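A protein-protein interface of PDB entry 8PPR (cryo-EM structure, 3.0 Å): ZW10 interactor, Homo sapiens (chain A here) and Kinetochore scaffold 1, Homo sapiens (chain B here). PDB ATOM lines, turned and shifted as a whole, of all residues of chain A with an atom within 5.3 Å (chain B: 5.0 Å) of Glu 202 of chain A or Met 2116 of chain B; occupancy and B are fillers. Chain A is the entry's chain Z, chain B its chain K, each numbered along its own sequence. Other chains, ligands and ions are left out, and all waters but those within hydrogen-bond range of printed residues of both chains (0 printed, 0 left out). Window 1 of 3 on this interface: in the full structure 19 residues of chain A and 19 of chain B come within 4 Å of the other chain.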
ATOM      1  N   GLN A 197     -10.686  12.553   3.195  1.00  0.00           N
ATOM      2  CA  GLN A 197     -11.783  13.290   2.573  1.00  0.00           C
ATOM      3  C   GLN A 197     -12.039  12.801   1.153  1.00  0.00           C
ATOM      4  O   GLN A 197     -13.195  12.647   0.736  1.00  0.00           O
ATOM      5  CB  GLN A 197     -11.481  14.788   2.579  1.00  0.00           C
ATOM      6  CG  GLN A 197     -12.660  15.654   2.172  1.00  0.00           C
ATOM      7  CD  GLN A 197     -12.356  17.134   2.271  1.00  0.00           C
ATOM      8  OE1 GLN A 197     -11.252  17.529   2.644  1.00  0.00           O
ATOM      9  NE2 GLN A 197     -13.337  17.963   1.935  1.00  0.00           N
ATOM     10  N   GLN A 198     -10.968  12.553   0.393  1.00  0.00           N
ATOM     11  CA  GLN A 198     -11.126  11.993  -0.947  1.00  0.00           C
ATOM     12  C   GLN A 198     -11.786  10.620  -0.892  1.00  0.00           C
ATOM     13  O   GLN A 198     -12.631  10.291  -1.733  1.00  0.00           O
ATOM     14  CB  GLN A 198      -9.767  11.903  -1.641  1.00  0.00           C
ATOM     15  CG  GLN A 198      -9.849  11.574  -3.122  1.00  0.00           C
ATOM     16  CD  GLN A 198      -8.493  11.595  -3.797  1.00  0.00           C
ATOM     17  OE1 GLN A 198      -7.462  11.758  -3.143  1.00  0.00           O
ATOM     18  NE2 GLN A 198      -8.485  11.428  -5.115  1.00  0.00           N
ATOM     19  N   ALA A 199     -11.402   9.803   0.091  1.00  0.00           N
ATOM     20  CA  ALA A 199     -12.002   8.484   0.249  1.00  0.00           C
ATOM     21  C   ALA A 199     -13.485   8.588   0.570  1.00  0.00           C
ATOM     22  O   ALA A 199     -14.294   7.815   0.049  1.00  0.00           O
ATOM     23  CB  ALA A 199     -11.267   7.701   1.337  1.00  0.00           C
ATOM     24  N   GLU A 200     -13.859   9.532   1.436  1.00  0.00           N
ATOM     25  CA  GLU A 200     -15.271   9.738   1.745  1.00  0.00           C
ATOM     26  C   GLU A 200     -16.045  10.184   0.512  1.00  0.00           C
ATOM     27  O   GLU A 200     -17.165   9.716   0.268  1.00  0.00           O
ATOM     28  CB  GLU A 200     -15.417  10.765   2.867  1.00  0.00           C
ATOM     29  CG  GLU A 200     -15.227  10.197   4.261  1.00  0.00           C
ATOM     30  CD  GLU A 200     -15.327  11.258   5.337  1.00  0.00           C
ATOM     31  OE1 GLU A 200     -15.570  12.433   4.991  1.00  0.00           O
ATOM     32  OE2 GLU A 200     -15.164  10.919   6.527  1.00  0.00           O
ATOM     33  N   GLN A 201     -15.463  11.090  -0.280  1.00  0.00           N
ATOM     34  CA  GLN A 201     -16.120  11.526  -1.508  1.00  0.00           C
ATOM     35  C   GLN A 201     -16.321  10.360  -2.468  1.00  0.00           C
ATOM     36  O   GLN A 201     -17.406  10.192  -3.041  1.00  0.00           O
ATOM     37  CB  GLN A 201     -15.303  12.637  -2.170  1.00  0.00           C
ATOM     38  CG  GLN A 201     -15.981  13.305  -3.357  1.00  0.00           C
ATOM     39  CD  GLN A 201     -15.750  12.563  -4.661  1.00  0.00           C
ATOM     40  OE1 GLN A 201     -14.722  11.908  -4.841  1.00  0.00           O
ATOM     41  NE2 GLN A 201     -16.709  12.658  -5.574  1.00  0.00           N
ATOM     42  N   GLU A 202     -15.289   9.536  -2.644  1.00  0.00           N
ATOM     43  CA  GLU A 202     -15.386   8.414  -3.570  1.00  0.00           C
ATOM     44  C   GLU A 202     -16.366   7.364  -3.056  1.00  0.00           C
ATOM     45  O   GLU A 202     -17.080   6.732  -3.842  1.00  0.00           O
ATOM     46  CB  GLU A 202     -13.999   7.814  -3.791  1.00  0.00           C
ATOM     47  CG  GLU A 202     -13.908   6.713  -4.834  1.00  0.00           C
ATOM     48  CD  GLU A 202     -14.171   7.217  -6.238  1.00  0.00           C
ATOM     49  OE1 GLU A 202     -13.945   8.418  -6.496  1.00  0.00           O
ATOM     50  OE2 GLU A 202     -14.564   6.404  -7.097  1.00  0.00           O
ATOM     51  N   ARG A 203     -16.425   7.173  -1.735  1.00  0.00           N
ATOM     52  CA  ARG A 203     -17.398   6.253  -1.156  1.00  0.00           C
ATOM     53  C   ARG A 203     -18.823   6.746  -1.378  1.00  0.00           C
ATOM     54  O   ARG A 203     -19.718   5.956  -1.703  1.00  0.00           O
ATOM     55  CB  ARG A 203     -17.123   6.079   0.336  1.00  0.00           C
ATOM     56  CG  ARG A 203     -17.923   4.970   0.995  1.00  0.00           C
ATOM     57  CD  ARG A 203     -17.642   4.921   2.486  1.00  0.00           C
ATOM     58  NE  ARG A 203     -18.390   5.949   3.200  1.00  0.00           N
ATOM     59  CZ  ARG A 203     -17.870   6.764   4.108  1.00  0.00           C
ATOM     60  NH1 ARG A 203     -16.591   6.702   4.440  1.00  0.00           N
ATOM     61  NH2 ARG A 203     -18.652   7.665   4.695  1.00  0.00           N
ATOM     62  N   ASP A 204     -19.053   8.049  -1.200  1.00  0.00           N
ATOM     63  CA  ASP A 204     -20.371   8.613  -1.474  1.00  0.00           C
ATOM     64  C   ASP A 204     -20.723   8.463  -2.948  1.00  0.00           C
ATOM     65  O   ASP A 204     -21.881   8.219  -3.302  1.00  0.00           O
ATOM     66  CB  ASP A 204     -20.399  10.086  -1.057  1.00  0.00           C
ATOM     67  CG  ASP A 204     -21.793  10.697  -1.111  1.00  0.00           C
ATOM     68  OD1 ASP A 204     -22.757  10.004  -1.500  1.00  0.00           O
ATOM     69  OD2 ASP A 204     -21.926  11.889  -0.765  1.00  0.00           O
ATOM     70  N   LYS A 205     -19.727   8.596  -3.822  1.00  0.00           N
ATOM     71  CA  LYS A 205     -19.985   8.527  -5.256  1.00  0.00           C
ATOM     72  C   LYS A 205     -20.108   7.076  -5.730  1.00  0.00           C
ATOM     73  O   LYS A 205     -20.600   6.824  -6.836  1.00  0.00           O
ATOM     74  CB  LYS A 205     -18.869   9.287  -5.980  1.00  0.00           C
ATOM     75  CG  LYS A 205     -18.942   9.354  -7.491  1.00  0.00           C
ATOM     76  CD  LYS A 205     -20.114  10.186  -7.969  1.00  0.00           C
ATOM     77  CE  LYS A 205     -20.056  10.362  -9.476  1.00  0.00           C
ATOM     78  NZ  LYS A 205     -20.249   9.071 -10.191  1.00  0.00           N
ATOM     79  N   LEU A 206     -19.678   6.116  -4.903  1.00  0.00           N
ATOM     80  CA  LEU A 206     -19.774   4.699  -5.259  1.00  0.00           C
ATOM     81  C   LEU A 206     -21.209   4.191  -5.222  1.00  0.00           C
ATOM     82  O   LEU A 206     -21.651   3.490  -6.147  1.00  0.00           O
ATOM     83  CB  LEU A 206     -18.904   3.867  -4.317  1.00  0.00           C
ATOM     84  CG  LEU A 206     -18.841   2.362  -4.589  1.00  0.00           C
ATOM     85  CD1 LEU A 206     -18.229   2.076  -5.951  1.00  0.00           C
ATOM     86  CD2 LEU A 206     -18.073   1.646  -3.487  1.00  0.00           C
ATOM     87  N   GLN B2112      -6.826   1.606  -0.301  1.00  0.00           N
ATOM     88  CA  GLN B2112      -8.284   1.561  -0.333  1.00  0.00           C
ATOM     89  C   GLN B2112      -8.836   2.421  -1.463  1.00  0.00           C
ATOM     90  O   GLN B2112      -9.804   2.037  -2.134  1.00  0.00           O
ATOM     91  CB  GLN B2112      -8.855   2.013   1.010  1.00  0.00           C
ATOM     92  CG  GLN B2112     -10.317   1.656   1.216  1.00  0.00           C
ATOM     93  CD  GLN B2112     -10.816   2.014   2.602  1.00  0.00           C
ATOM     94  OE1 GLN B2112     -10.275   2.904   3.258  1.00  0.00           O
ATOM     95  NE2 GLN B2112     -11.857   1.324   3.054  1.00  0.00           N
ATOM     96  N   ILE B2113      -8.237   3.594  -1.681  1.00  0.00           N
ATOM     97  CA  ILE B2113      -8.674   4.471  -2.764  1.00  0.00           C
ATOM     98  C   ILE B2113      -8.504   3.779  -4.108  1.00  0.00           C
ATOM     99  O   ILE B2113      -9.409   3.794  -4.952  1.00  0.00           O
ATOM    100  CB  ILE B2113      -7.907   5.807  -2.712  1.00  0.00           C
ATOM    101  CG1 ILE B2113      -8.348   6.635  -1.504  1.00  0.00           C
ATOM    102  CG2 ILE B2113      -8.117   6.594  -3.998  1.00  0.00           C
ATOM    103  CD1 ILE B2113      -7.491   7.854  -1.250  1.00  0.00           C
ATOM    104  N   ASP B2114      -7.345   3.153  -4.323  1.00  0.00           N
ATOM    105  CA  ASP B2114      -7.111   2.441  -5.576  1.00  0.00           C
ATOM    106  C   ASP B2114      -8.088   1.283  -5.745  1.00  0.00           C
ATOM    107  O   ASP B2114      -8.612   1.059  -6.843  1.00  0.00           O
ATOM    108  CB  ASP B2114      -5.669   1.939  -5.634  1.00  0.00           C
ATOM    109  CG  ASP B2114      -5.279   1.451  -7.014  1.00  0.00           C
ATOM    110  OD1 ASP B2114      -5.404   2.233  -7.980  1.00  0.00           O
ATOM    111  OD2 ASP B2114      -4.848   0.285  -7.133  1.00  0.00           O
ATOM    112  N   PHE B2115      -8.349   0.541  -4.666  1.00  0.00           N
ATOM    113  CA  PHE B2115      -9.275  -0.584  -4.747  1.00  0.00           C
ATOM    114  C   PHE B2115     -10.681  -0.127  -5.119  1.00  0.00           C
ATOM    115  O   PHE B2115     -11.328  -0.726  -5.988  1.00  0.00           O
ATOM    116  CB  PHE B2115      -9.300  -1.340  -3.420  1.00  0.00           C
ATOM    117  CG  PHE B2115     -10.327  -2.433  -3.367  1.00  0.00           C
ATOM    118  CD1 PHE B2115     -10.147  -3.609  -4.074  1.00  0.00           C
ATOM    119  CD2 PHE B2115     -11.480  -2.279  -2.615  1.00  0.00           C
ATOM    120  CE1 PHE B2115     -11.094  -4.614  -4.028  1.00  0.00           C
ATOM    121  CE2 PHE B2115     -12.432  -3.280  -2.566  1.00  0.00           C
ATOM    122  CZ  PHE B2115     -12.238  -4.449  -3.273  1.00  0.00           C
ATOM    123  N   MET B2116     -11.171   0.935  -4.478  1.00  0.00           N
ATOM    124  CA  MET B2116     -12.529   1.383  -4.769  1.00  0.00           C
ATOM    125  C   MET B2116     -12.616   2.041  -6.141  1.00  0.00           C
ATOM    126  O   MET B2116     -13.653   1.964  -6.805  1.00  0.00           O
ATOM    127  CB  MET B2116     -13.034   2.312  -3.666  1.00  0.00           C
ATOM    128  CG  MET B2116     -12.250   3.586  -3.477  1.00  0.00           C
ATOM    129  SD  MET B2116     -12.871   4.483  -2.046  1.00  0.00           S
ATOM    130  CE  MET B2116     -11.770   5.883  -2.037  1.00  0.00           C
ATOM    131  N   GLN B2117     -11.530   2.671  -6.599  1.00  0.00           N
ATOM    132  CA  GLN B2117     -11.513   3.188  -7.965  1.00  0.00           C
ATOM    133  C   GLN B2117     -11.562   2.056  -8.986  1.00  0.00           C
ATOM    134  O   GLN B2117     -12.250   2.157 -10.011  1.00  0.00           O
ATOM    135  CB  GLN B2117     -10.277   4.063  -8.173  1.00  0.00           C
ATOM    136  CG  GLN B2117     -10.403   5.445  -7.548  1.00  0.00           C
ATOM    137  CD  GLN B2117      -9.149   6.279  -7.702  1.00  0.00           C
ATOM    138  OE1 GLN B2117      -8.058   5.749  -7.912  1.00  0.00           O
ATOM    139  NE2 GLN B2117      -9.296   7.594  -7.592  1.00  0.00           N
ATOM    140  N   LYS B2118     -10.837   0.964  -8.724  1.00  0.00           N
ATOM    141  CA  LYS B2118     -10.905  -0.199  -9.606  1.00  0.00           C
ATOM    142  C   LYS B2118     -12.302  -0.808  -9.602  1.00  0.00           C
ATOM    143  O   LYS B2118     -12.817  -1.218 -10.651  1.00  0.00           O
ATOM    144  CB  LYS B2118      -9.861  -1.232  -9.183  1.00  0.00           C
ATOM    145  CG  LYS B2118      -8.449  -0.901  -9.636  1.00  0.00           C
ATOM    146  CD  LYS B2118      -7.463  -1.982  -9.225  1.00  0.00           C
ATOM    147  CE  LYS B2118      -6.044  -1.611  -9.626  1.00  0.00           C
ATOM    148  NZ  LYS B2118      -5.044  -2.592  -9.123  1.00  0.00           N
ATOM    149  N   GLN B2119     -12.928  -0.878  -8.425  1.00  0.00           N
ATOM    150  CA  GLN B2119     -14.308  -1.350  -8.345  1.00  0.00           C
ATOM    151  C   GLN B2119     -15.238  -0.444  -9.142  1.00  0.00           C
ATOM    152  O   GLN B2119     -16.163  -0.921  -9.809  1.00  0.00           O
ATOM    153  CB  GLN B2119     -14.753  -1.426  -6.885  1.00  0.00           C
ATOM    154  CG  GLN B2119     -14.189  -2.613  -6.123  1.00  0.00           C
ATOM    155  CD  GLN B2119     -14.620  -3.942  -6.709  1.00  0.00           C
ATOM    156  OE1 GLN B2119     -15.807  -4.270  -6.729  1.00  0.00           O
ATOM    157  NE2 GLN B2119     -13.655  -4.717  -7.189  1.00  0.00           N
ATOM    158  N   ARG B2120     -15.006   0.869  -9.077  1.00  0.00           N
ATOM    159  CA  ARG B2120     -15.789   1.816  -9.863  1.00  0.00           C
ATOM    160  C   ARG B2120     -15.650   1.541 -11.350  1.00  0.00           C
ATOM    161  O   ARG B2120     -16.640   1.553 -12.091  1.00  0.00           O
ATOM    162  CB  ARG B2120     -15.324   3.239  -9.578  1.00  0.00           C
ATOM    163  CG  ARG B2120     -16.230   4.289 -10.157  1.00  0.00           C
ATOM    164  CD  ARG B2120     -17.558   4.234  -9.454  1.00  0.00           C
ATOM    165  NE  ARG B2120     -17.310   4.430  -8.033  1.00  0.00           N
ATOM    166  CZ  ARG B2120     -17.286   5.620  -7.452  1.00  0.00           C
ATOM    167  NH1 ARG B2120     -17.525   6.722  -8.138  1.00  0.00           N
ATOM    168  NH2 ARG B2120     -16.964   5.710  -6.165  1.00  0.00           N
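NH1 of Arg 2120 of chain B sits close to O of Lys 205 of chain A, 3.3 Å away.
N of Leu 206 of chain A sits close to NH2 of Arg 2120 of chain B, at 3.0 Å.
The guanidinium group (NH2) of Arg 2120 of chain B lies within salt-bridge range of the side-chain carboxylate (OE2) of Glu 202 of chain A (2.7 Å).
Among the printed residues, merely in contact across the chains: Ala 199 of chain A with Met 2116 of chain B and Glu 202 of chain A with Met 2116 of chain B.
Of chain B, only Met 2116 and Arg 2120 come within 4 Å of Glu 202 of chain A.
Met 2116 of chain B touches two residues of chain A.
Of the printed residues of chain B, Leu 206 of chain A touches Arg 2120.
Printed residues of chain A within 4 Å of Arg 2120 of chain B: Glu 202, Lys 205 and Leu 206.
Of the printed residues of chain B, Ala 199 of chain A touches Met 2116 (3.5 Å).
Of the printed residues of chain B, Lys 205 of chain A touches Arg 2120 (3.1 Å).
The nearest residue of chain B that does not touch Glu 202 of chain A is Gln 2117 of chain B (4.3 Å).
The nearest residue of chain A that does not touch Met 2116 of chain B is Arg 203 of chain A (4.5 Å).
The nearest printed residue of chain A that does not touch Arg 2120 of chain B is Arg 203 of chain A (4.7 Å).
Of the 10 printed residues of chain A, 4 touch a printed residue of chain B.
Printed residues of chain A that touch a printed residue of chain B: Ala 199, Glu 202, Lys 205 and Leu 206.
Hydrophobic or aromatic side chains of chain A within 4 Å of the printed part of chain B: Ala 199 and Leu 206.
Printed residues of chain B that touch a printed residue of chain A: Met 2116 and Arg 2120.
Among the printed residues, 5 pairs touch across the chains.
Among the printed residues, Asp or Glu carboxylates within 4 Å of a Lys or Arg side-chain nitrogen of the other chain: Glu 202 of chain A with Arg 2120 of chain B.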
